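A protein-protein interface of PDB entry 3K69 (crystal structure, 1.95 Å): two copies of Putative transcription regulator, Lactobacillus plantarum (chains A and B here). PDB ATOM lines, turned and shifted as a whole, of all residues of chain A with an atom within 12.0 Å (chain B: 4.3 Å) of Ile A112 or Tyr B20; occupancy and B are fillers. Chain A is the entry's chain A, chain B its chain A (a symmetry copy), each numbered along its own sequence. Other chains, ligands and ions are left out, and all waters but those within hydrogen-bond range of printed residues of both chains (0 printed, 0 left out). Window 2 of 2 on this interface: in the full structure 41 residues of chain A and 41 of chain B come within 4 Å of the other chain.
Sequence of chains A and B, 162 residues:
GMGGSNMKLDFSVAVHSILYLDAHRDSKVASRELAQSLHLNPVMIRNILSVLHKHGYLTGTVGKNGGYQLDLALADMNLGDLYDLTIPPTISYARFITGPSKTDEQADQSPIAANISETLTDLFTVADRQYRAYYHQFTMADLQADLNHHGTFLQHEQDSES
Of the 13 printed residues of chain B, 4 touch a printed residue of chain A. Hydrophobic or aromatic side chains of chain B that line the printed part of chain A: His B16. Along chain B the printed residues that touch a printed residue of chain A span positions 16 to 37. Of the 21 printed residues of chain A, 3 touch a printed residue of chain B. Hydrophobic or aromatic side chains of chain A within 4 Å of the printed part of chain B: Ile A112. Among the printed residues, no Asp or Glu carboxylate lies within 4 Å of a Lys or Arg side-chain nitrogen of the other chain.
ND1 of His B16 is in hydrogen-bond range of OG1 of Thr A98, at 2.6 Å.
A ring nitrogen (NE2) of His B16 lies within hydrogen-bond range of the side-chain hydroxyl (OG) of Ser B37 (3.2 Å). The side-chain hydroxyl (OH) of Tyr B20 lies within hydrogen-bond range of the side-chain carboxylate (OE2) of Glu B33 (2.6 Å). The backbone NH (N) of Ile A112 sits close to the side-chain hydroxyl (OG) of Ser A110. O of Tyr B20 lies within hydrogen-bond range of ND1 of His B24, 3.1 Å away.
Ile A112 touches three residues of chain B. Tyr B20 touches just one residue of chain A: Ile A112. Of the printed residues of chain A, His B16 touches Thr A98, Gly A99 and Ile A112. No residue of chain A comes within 4 Å of Leu B21. Asp B22 touches none of the printed residues of chain A. No residue of chain A comes within 4 Å of Ala B23. No residue of chain A comes within 4 Å of His B24. No residue of chain A comes within 4 Å of Val B29. No residue of chain A comes within 4 Å of Glu B33. No residue of chain A comes within 4 Å of Leu B34. Ser B37 touches one residue of chain A. Of the printed residues of chain B, Gly A99 touches His B16 and Ser B37. Of the printed residues of chain A, Leu B19 touches Ile A112 (3.6 Å). Printed residues of chain B within 4 Å of Thr A98: His B16 (2.6 Å). The nearest printed residue of chain B that does not touch Ile A112 is Ala B23 (4.5 Å). The nearest residue of chain A that does not touch Tyr B20 is Ser A110 (6.0 Å). The nearest printed residue of chain A that does not touch Leu B19 is Ile A116 (4.01 Å).
Among the printed residues, merely in contact across the chains: Gly A99 with His B16, Gly A99 with Ser B37, Ile A112 with His B16, Ile A112 with Leu B19 and Ile A112 with Tyr B20.
No position is printed for both chains.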
ATOM      1  N   ILE A  97     -18.390   4.913   1.785  1.00  0.00           N
ATOM      2  CA  ILE A  97     -18.599   6.294   1.411  1.00  0.00           C
ATOM      3  C   ILE A  97     -20.112   6.627   1.343  1.00  0.00           C
ATOM      4  O   ILE A  97     -20.940   5.855   0.812  1.00  0.00           O
ATOM      5  CB  ILE A  97     -17.859   6.599   0.075  1.00  0.00           C
ATOM      6  CG1 ILE A  97     -16.341   6.372   0.241  1.00  0.00           C
ATOM      7  CG2 ILE A  97     -18.279   7.976  -0.501  1.00  0.00           C
ATOM      8  CD1 ILE A  97     -15.585   6.402  -1.077  1.00  0.00           C
ATOM      9  N   THR A  98     -20.446   7.793   1.889  1.00  0.00           N
ATOM     10  CA  THR A  98     -21.822   8.361   1.945  1.00  0.00           C
ATOM     11  C   THR A  98     -22.181   9.226   0.707  1.00  0.00           C
ATOM     12  O   THR A  98     -21.364   9.389  -0.205  1.00  0.00           O
ATOM     13  CB  THR A  98     -21.974   9.268   3.227  1.00  0.00           C
ATOM     14  OG1 THR A  98     -20.980  10.310   3.186  1.00  0.00           O
ATOM     15  CG2 THR A  98     -21.847   8.429   4.551  1.00  0.00           C
ATOM     16  N   GLY A  99     -23.385   9.800   0.684  1.00  0.00           N
ATOM     17  CA  GLY A  99     -23.838  10.625  -0.450  1.00  0.00           C
ATOM     18  C   GLY A  99     -24.426   9.763  -1.571  1.00  0.00           C
ATOM     19  O   GLY A  99     -24.804   8.605  -1.314  1.00  0.00           O
ATOM     20  N   PRO A 100     -24.504  10.314  -2.819  1.00  0.00           N
ATOM     21  CA  PRO A 100     -24.932   9.578  -4.022  1.00  0.00           C
ATOM     22  C   PRO A 100     -23.873   8.656  -4.678  1.00  0.00           C
ATOM     23  O   PRO A 100     -22.690   8.672  -4.318  1.00  0.00           O
ATOM     24  CB  PRO A 100     -25.287  10.711  -4.995  1.00  0.00           C
ATOM     25  CG  PRO A 100     -24.292  11.731  -4.698  1.00  0.00           C
ATOM     26  CD  PRO A 100     -24.201  11.716  -3.169  1.00  0.00           C
ATOM     27  N   SER A 101     -24.339   7.879  -5.654  1.00  0.00           N
ATOM     28  CA  SER A 101     -23.511   6.961  -6.453  1.00  0.00           C
ATOM     29  C   SER A 101     -23.359   7.458  -7.918  1.00  0.00           C
ATOM     30  O   SER A 101     -23.966   8.476  -8.305  1.00  0.00           O
ATOM     31  CB  SER A 101     -24.148   5.567  -6.423  1.00  0.00           C
ATOM     32  OG  SER A 101     -25.533   5.666  -6.721  1.00  0.00           O
ATOM     33  N   LYS A 102     -22.563   6.741  -8.722  1.00  0.00           N
ATOM     34  CA  LYS A 102     -22.260   7.151 -10.112  1.00  0.00           C
ATOM     35  C   LYS A 102     -23.391   6.844 -11.112  1.00  0.00           C
ATOM     36  O   LYS A 102     -24.545   7.258 -10.940  1.00  0.00           O
ATOM     37  CB  LYS A 102     -20.951   6.498 -10.586  1.00  0.00           C
ATOM     38  N   ALA A 107     -25.328  16.804 -11.306  1.00  0.00           N
ATOM     39  CA  ALA A 107     -25.759  18.045 -11.991  1.00  0.00           C
ATOM     40  C   ALA A 107     -26.481  19.013 -11.043  1.00  0.00           C
ATOM     41  O   ALA A 107     -26.234  20.225 -11.085  1.00  0.00           O
ATOM     42  CB  ALA A 107     -26.640  17.725 -13.194  1.00  0.00           C
ATOM     43  N   ASP A 108     -27.396  18.474 -10.226  1.00  0.00           N
ATOM     44  CA  ASP A 108     -27.914  19.172  -9.029  1.00  0.00           C
ATOM     45  C   ASP A 108     -27.449  18.439  -7.771  1.00  0.00           C
ATOM     46  O   ASP A 108     -28.084  18.533  -6.719  1.00  0.00           O
ATOM     47  CB  ASP A 108     -29.446  19.294  -9.017  1.00  0.00           C
ATOM     48  N   GLN A 109     -26.343  17.706  -7.875  1.00  0.00           N
ATOM     49  CA  GLN A 109     -25.629  17.306  -6.687  1.00  0.00           C
ATOM     50  C   GLN A 109     -25.125  18.564  -5.996  1.00  0.00           C
ATOM     51  O   GLN A 109     -24.609  19.481  -6.644  1.00  0.00           O
ATOM     52  CB  GLN A 109     -24.461  16.366  -7.011  1.00  0.00           C
ATOM     53  CG  GLN A 109     -24.870  14.912  -7.238  1.00  0.00           C
ATOM     54  CD  GLN A 109     -26.156  14.557  -6.506  1.00  0.00           C
ATOM     55  OE1 GLN A 109     -26.163  14.359  -5.288  1.00  0.00           O
ATOM     56  NE2 GLN A 109     -27.264  14.507  -7.251  1.00  0.00           N
ATOM     57  N   SER A 110     -25.310  18.616  -4.677  1.00  0.00           N
ATOM     58  CA  SER A 110     -24.714  19.663  -3.871  1.00  0.00           C
ATOM     59  C   SER A 110     -23.210  19.531  -4.012  1.00  0.00           C
ATOM     60  O   SER A 110     -22.707  18.446  -4.301  1.00  0.00           O
ATOM     61  CB  SER A 110     -25.102  19.534  -2.386  1.00  0.00           C
ATOM     62  OG  SER A 110     -24.422  18.458  -1.733  1.00  0.00           O
ATOM     63  N   PRO A 111     -22.491  20.635  -3.815  1.00  0.00           N
ATOM     64  CA  PRO A 111     -21.040  20.577  -3.742  1.00  0.00           C
ATOM     65  C   PRO A 111     -20.514  19.356  -2.948  1.00  0.00           C
ATOM     66  O   PRO A 111     -19.629  18.663  -3.432  1.00  0.00           O
ATOM     67  CB  PRO A 111     -20.679  21.896  -3.056  1.00  0.00           C
ATOM     68  CG  PRO A 111     -21.770  22.856  -3.516  1.00  0.00           C
ATOM     69  CD  PRO A 111     -23.011  22.010  -3.655  1.00  0.00           C
ATOM     70  N   ILE A 112     -21.088  19.070  -1.785  1.00  0.00           N
ATOM     71  CA  ILE A 112     -20.572  18.005  -0.917  1.00  0.00           C
ATOM     72  C   ILE A 112     -20.870  16.671  -1.540  1.00  0.00           C
ATOM     73  O   ILE A 112     -19.970  15.888  -1.766  1.00  0.00           O
ATOM     74  CB  ILE A 112     -21.154  18.033   0.522  1.00  0.00           C
ATOM     75  CG1 ILE A 112     -20.810  19.348   1.219  1.00  0.00           C
ATOM     76  CG2 ILE A 112     -20.628  16.884   1.340  1.00  0.00           C
ATOM     77  CD1 ILE A 112     -21.829  19.751   2.200  1.00  0.00           C
ATOM     78  N   ALA A 113     -22.145  16.427  -1.832  1.00  0.00           N
ATOM     79  CA  ALA A 113     -22.573  15.178  -2.462  1.00  0.00           C
ATOM     80  C   ALA A 113     -21.866  14.866  -3.777  1.00  0.00           C
ATOM     81  O   ALA A 113     -21.616  13.720  -4.063  1.00  0.00           O
ATOM     82  CB  ALA A 113     -24.075  15.200  -2.696  1.00  0.00           C
ATOM     83  N   ALA A 114     -21.564  15.886  -4.578  1.00  0.00           N
ATOM     84  CA  ALA A 114     -20.961  15.678  -5.903  1.00  0.00           C
ATOM     85  C   ALA A 114     -19.494  15.262  -5.819  1.00  0.00           C
ATOM     86  O   ALA A 114     -18.962  14.704  -6.752  1.00  0.00           O
ATOM     87  CB  ALA A 114     -21.070  16.959  -6.726  1.00  0.00           C
ATOM     88  N   ASN A 115     -18.845  15.595  -4.709  1.00  0.00           N
ATOM     89  CA  ASN A 115     -17.379  15.555  -4.590  1.00  0.00           C
ATOM     90  C   ASN A 115     -16.820  14.607  -3.543  1.00  0.00           C
ATOM     91  O   ASN A 115     -15.639  14.297  -3.559  1.00  0.00           O
ATOM     92  CB  ASN A 115     -16.885  16.962  -4.278  1.00  0.00           C
ATOM     93  CG  ASN A 115     -17.001  17.890  -5.482  1.00  0.00           C
ATOM     94  OD1 ASN A 115     -16.440  17.614  -6.544  1.00  0.00           O
ATOM     95  ND2 ASN A 115     -17.757  18.978  -5.331  1.00  0.00           N
ATOM     96  N   ILE A 116     -17.667  14.199  -2.609  1.00  0.00           N
ATOM     97  CA  ILE A 116     -17.250  13.407  -1.466  1.00  0.00           C
ATOM     98  C   ILE A 116     -16.686  12.057  -1.871  1.00  0.00           C
ATOM     99  O   ILE A 116     -15.674  11.600  -1.325  1.00  0.00           O
ATOM    100  CB  ILE A 116     -18.415  13.306  -0.413  1.00  0.00           C
ATOM    101  CG1 ILE A 116     -17.951  12.647   0.881  1.00  0.00           C
ATOM    102  CG2 ILE A 116     -19.594  12.517  -0.931  1.00  0.00           C
ATOM    103  CD1 ILE A 116     -17.092  13.493   1.719  1.00  0.00           C
ATOM    104  N   SER A 117     -17.309  11.398  -2.840  1.00  0.00           N
ATOM    105  CA  SER A 117     -16.846  10.067  -3.204  1.00  0.00           C
ATOM    106  C   SER A 117     -15.433  10.137  -3.759  1.00  0.00           C
ATOM    107  O   SER A 117     -14.573   9.341  -3.387  1.00  0.00           O
ATOM    108  CB  SER A 117     -17.794   9.372  -4.180  1.00  0.00           C
ATOM    109  OG  SER A 117     -17.247   8.121  -4.517  1.00  0.00           O
ATOM    110  N   GLU A 118     -15.155  11.125  -4.608  1.00  0.00           N
ATOM    111  CA  GLU A 118     -13.810  11.188  -5.181  1.00  0.00           C
ATOM    112  C   GLU A 118     -12.742  11.573  -4.145  1.00  0.00           C
ATOM    113  O   GLU A 118     -11.660  11.033  -4.167  1.00  0.00           O
ATOM    114  CB  GLU A 118     -13.738  12.116  -6.390  1.00  0.00           C
ATOM    115  CG  GLU A 118     -12.346  12.160  -7.006  1.00  0.00           C
ATOM    116  CD  GLU A 118     -12.231  13.167  -8.144  1.00  0.00           C
ATOM    117  OE1 GLU A 118     -13.267  13.769  -8.502  1.00  0.00           O
ATOM    118  OE2 GLU A 118     -11.100  13.316  -8.669  1.00  0.00           O
ATOM    119  N   THR A 119     -13.053  12.523  -3.267  1.00  0.00           N
ATOM    120  CA  THR A 119     -12.175  12.907  -2.153  1.00  0.00           C
ATOM    121  C   THR A 119     -11.852  11.786  -1.158  1.00  0.00           C
ATOM    122  O   THR A 119     -10.684  11.546  -0.810  1.00  0.00           O
ATOM    123  CB  THR A 119     -12.818  14.076  -1.394  1.00  0.00           C
ATOM    124  OG1 THR A 119     -12.742  15.223  -2.244  1.00  0.00           O
ATOM    125  CG2 THR A 119     -12.090  14.368   0.005  1.00  0.00           C
ATOM    126  N   LEU A 120     -12.875  11.069  -0.718  1.00  0.00           N
ATOM    127  CA  LEU A 120     -12.659   9.944   0.201  1.00  0.00           C
ATOM    128  C   LEU A 120     -11.982   8.776  -0.428  1.00  0.00           C
ATOM    129  O   LEU A 120     -11.154   8.118   0.213  1.00  0.00           O
ATOM    130  CB  LEU A 120     -13.957   9.518   0.894  1.00  0.00           C
ATOM    131  CG  LEU A 120     -14.467  10.517   1.923  1.00  0.00           C
ATOM    132  CD1 LEU A 120     -15.828  10.029   2.399  1.00  0.00           C
ATOM    133  CD2 LEU A 120     -13.455  10.710   3.107  1.00  0.00           C
ATOM    134  N   THR A 121     -12.314   8.508  -1.693  1.00  0.00           N
ATOM    135  CA  THR A 121     -11.633   7.471  -2.436  1.00  0.00           C
ATOM    136  C   THR A 121     -10.129   7.767  -2.509  1.00  0.00           C
ATOM    137  O   THR A 121      -9.317   6.885  -2.260  1.00  0.00           O
ATOM    138  CB  THR A 121     -12.221   7.249  -3.860  1.00  0.00           C
ATOM    139  OG1 THR A 121     -13.585   6.864  -3.743  1.00  0.00           O
ATOM    140  CG2 THR A 121     -11.437   6.141  -4.641  1.00  0.00           C
ATOM    141  N   HIS B  16     -18.949  13.696   6.237  1.00  0.00           N
ATOM    142  CA  HIS B  16     -20.045  14.253   5.453  1.00  0.00           C
ATOM    143  C   HIS B  16     -20.959  15.169   6.329  1.00  0.00           C
ATOM    144  O   HIS B  16     -21.351  16.278   5.908  1.00  0.00           O
ATOM    145  CB  HIS B  16     -20.818  13.107   4.808  1.00  0.00           C
ATOM    146  CG  HIS B  16     -21.699  13.519   3.689  1.00  0.00           C
ATOM    147  ND1 HIS B  16     -22.012  12.676   2.641  1.00  0.00           N
ATOM    148  CD2 HIS B  16     -22.343  14.689   3.445  1.00  0.00           C
ATOM    149  CE1 HIS B  16     -22.820  13.311   1.807  1.00  0.00           C
ATOM    150  NE2 HIS B  16     -23.026  14.538   2.267  1.00  0.00           N
ATOM    151  N   SER B  17     -21.243  14.740   7.566  1.00  0.00           N
ATOM    152  CA  SER B  17     -22.087  15.526   8.456  1.00  0.00           C
ATOM    153  C   SER B  17     -21.427  16.854   8.850  1.00  0.00           C
ATOM    154  O   SER B  17     -22.069  17.922   8.815  1.00  0.00           O
ATOM    155  CB  SER B  17     -22.478  14.703   9.703  1.00  0.00           C
ATOM    156  OG  SER B  17     -23.299  13.595   9.354  1.00  0.00           O
ATOM    157  N   ILE B  18     -20.149  16.801   9.226  1.00  0.00           N
ATOM    158  CA  ILE B  18     -19.391  18.030   9.501  1.00  0.00           C
ATOM    159  C   ILE B  18     -19.375  18.970   8.294  1.00  0.00           C
ATOM    160  O   ILE B  18     -19.572  20.171   8.443  1.00  0.00           O
ATOM    161  CB  ILE B  18     -17.959  17.741   9.991  1.00  0.00           C
ATOM    162  CG1 ILE B  18     -18.034  16.950  11.313  1.00  0.00           C
ATOM    163  CG2 ILE B  18     -17.200  19.071  10.182  1.00  0.00           C
ATOM    164  CD1 ILE B  18     -16.725  16.248  11.740  1.00  0.00           C
ATOM    165  N   LEU B  19     -19.133  18.441   7.103  1.00  0.00           N
ATOM    166  CA  LEU B  19     -19.142  19.298   5.918  1.00  0.00           C
ATOM    167  C   LEU B  19     -20.528  19.922   5.684  1.00  0.00           C
ATOM    168  O   LEU B  19     -20.643  21.095   5.344  1.00  0.00           O
ATOM    169  CB  LEU B  19     -18.663  18.552   4.684  1.00  0.00           C
ATOM    170  CG  LEU B  19     -17.201  18.112   4.663  1.00  0.00           C
ATOM    171  CD1 LEU B  19     -17.074  17.029   3.608  1.00  0.00           C
ATOM    172  CD2 LEU B  19     -16.285  19.263   4.418  1.00  0.00           C
ATOM    173  N   TYR B  20     -21.577  19.154   5.918  1.00  0.00           N
ATOM    174  CA  TYR B  20     -22.924  19.641   5.708  1.00  0.00           C
ATOM    175  C   TYR B  20     -23.228  20.769   6.690  1.00  0.00           C
ATOM    176  O   TYR B  20     -23.713  21.854   6.289  1.00  0.00           O
ATOM    177  CB  TYR B  20     -23.953  18.531   5.844  1.00  0.00           C
ATOM    178  CG  TYR B  20     -25.344  18.980   5.461  1.00  0.00           C
ATOM    179  CD1 TYR B  20     -25.778  18.880   4.133  1.00  0.00           C
ATOM    180  CD2 TYR B  20     -26.216  19.541   6.405  1.00  0.00           C
ATOM    181  CE1 TYR B  20     -27.062  19.296   3.744  1.00  0.00           C
ATOM    182  CE2 TYR B  20     -27.518  19.977   6.019  1.00  0.00           C
ATOM    183  CZ  TYR B  20     -27.930  19.829   4.693  1.00  0.00           C
ATOM    184  OH  TYR B  20     -29.183  20.254   4.278  1.00  0.00           O
ATOM    185  N   LEU B  21     -22.901  20.528   7.961  1.00  0.00           N
ATOM    186  CA  LEU B  21     -23.103  21.543   8.995  1.00  0.00           C
ATOM    187  C   LEU B  21     -22.260  22.830   8.758  1.00  0.00           C
ATOM    188  O   LEU B  21     -22.724  23.928   9.037  1.00  0.00           O
ATOM    189  CB  LEU B  21     -22.881  20.947  10.383  1.00  0.00           C
ATOM    190  CG  LEU B  21     -23.895  19.848  10.778  1.00  0.00           C
ATOM    191  CD1 LEU B  21     -23.514  19.134  12.037  1.00  0.00           C
ATOM    192  CD2 LEU B  21     -25.347  20.345  10.847  1.00  0.00           C
ATOM    193  N   ASP B  22     -21.055  22.678   8.221  1.00  0.00           N
ATOM    194  CA  ASP B  22     -20.196  23.806   7.850  1.00  0.00           C
ATOM    195  C   ASP B  22     -20.882  24.659   6.764  1.00  0.00           C
ATOM    196  O   ASP B  22     -20.631  25.840   6.708  1.00  0.00           O
ATOM    197  CB  ASP B  22     -18.837  23.289   7.328  1.00  0.00           C
ATOM    198  CG  ASP B  22     -17.914  24.396   6.848  1.00  0.00           C
ATOM    199  OD1 ASP B  22     -17.377  25.123   7.713  1.00  0.00           O
ATOM    200  OD2 ASP B  22     -17.715  24.524   5.620  1.00  0.00           O
ATOM    201  N   ALA B  23     -21.725  24.061   5.919  1.00  0.00           N
ATOM    202  CA  ALA B  23     -22.420  24.805   4.841  1.00  0.00           C
ATOM    203  C   ALA B  23     -23.667  25.490   5.361  1.00  0.00           C
ATOM    204  O   ALA B  23     -24.289  26.274   4.667  1.00  0.00           O
ATOM    205  CB  ALA B  23     -22.763  23.863   3.640  1.00  0.00           C
ATOM    206  N   HIS B  24     -24.046  25.221   6.605  1.00  0.00           N
ATOM    207  CA  HIS B  24     -25.301  25.715   7.131  1.00  0.00           C
ATOM    208  C   HIS B  24     -25.109  26.196   8.564  1.00  0.00           C
ATOM    209  O   HIS B  24     -25.886  25.850   9.447  1.00  0.00           O
ATOM    210  CB  HIS B  24     -26.342  24.600   7.062  1.00  0.00           C
ATOM    211  CG  HIS B  24     -26.748  24.246   5.669  1.00  0.00           C
ATOM    212  ND1 HIS B  24     -26.208  23.175   4.981  1.00  0.00           N
ATOM    213  CD2 HIS B  24     -27.592  24.858   4.811  1.00  0.00           C
ATOM    214  CE1 HIS B  24     -26.729  23.135   3.765  1.00  0.00           C
ATOM    215  NE2 HIS B  24     -27.579  24.137   3.644  1.00  0.00           N
ATOM    216  N   VAL B  29     -29.702  21.835  12.306  1.00  0.00           N
ATOM    217  CA  VAL B  29     -30.021  20.804  11.341  1.00  0.00           C
ATOM    218  C   VAL B  29     -30.366  19.516  12.082  1.00  0.00           C
ATOM    219  O   VAL B  29     -29.512  18.912  12.745  1.00  0.00           O
ATOM    220  CB  VAL B  29     -28.830  20.577  10.383  1.00  0.00           C
ATOM    221  CG1 VAL B  29     -29.175  19.519   9.329  1.00  0.00           C
ATOM    222  CG2 VAL B  29     -28.396  21.931   9.723  1.00  0.00           C
ATOM    223  N   GLU B  33     -32.728  15.864   8.215  1.00  0.00           N
ATOM    224  CA  GLU B  33     -32.132  16.658   7.157  1.00  0.00           C
ATOM    225  C   GLU B  33     -30.740  16.155   6.777  1.00  0.00           C
ATOM    226  O   GLU B  33     -30.409  16.038   5.602  1.00  0.00           O
ATOM    227  CB  GLU B  33     -32.077  18.133   7.582  1.00  0.00           C
ATOM    228  CG  GLU B  33     -31.486  19.025   6.514  1.00  0.00           C
ATOM    229  CD  GLU B  33     -31.499  20.512   6.833  1.00  0.00           C
ATOM    230  OE1 GLU B  33     -32.324  20.961   7.653  1.00  0.00           O
ATOM    231  OE2 GLU B  33     -30.647  21.225   6.254  1.00  0.00           O
ATOM    232  N   LEU B  34     -29.914  15.874   7.780  1.00  0.00           N
ATOM    233  CA  LEU B  34     -28.605  15.275   7.547  1.00  0.00           C
ATOM    234  C   LEU B  34     -28.739  13.916   6.847  1.00  0.00           C
ATOM    235  O   LEU B  34     -27.985  13.623   5.893  1.00  0.00           O
ATOM    236  CB  LEU B  34     -27.812  15.131   8.847  1.00  0.00           C
ATOM    237  CG  LEU B  34     -27.172  16.383   9.452  1.00  0.00           C
ATOM    238  CD1 LEU B  34     -26.849  16.183  10.933  1.00  0.00           C
ATOM    239  CD2 LEU B  34     -25.888  16.794   8.695  1.00  0.00           C
ATOM    240  N   SER B  37     -29.222  14.212   3.127  1.00  0.00           N
ATOM    241  CA  SER B  37     -27.939  14.486   2.454  1.00  0.00           C
ATOM    242  C   SER B  37     -26.990  13.267   2.406  1.00  0.00           C
ATOM    243  O   SER B  37     -26.343  13.024   1.397  1.00  0.00           O
ATOM    244  CB  SER B  37     -27.222  15.688   3.108  1.00  0.00           C
ATOM    245  OG  SER B  37     -25.885  15.860   2.630  1.00  0.00           O
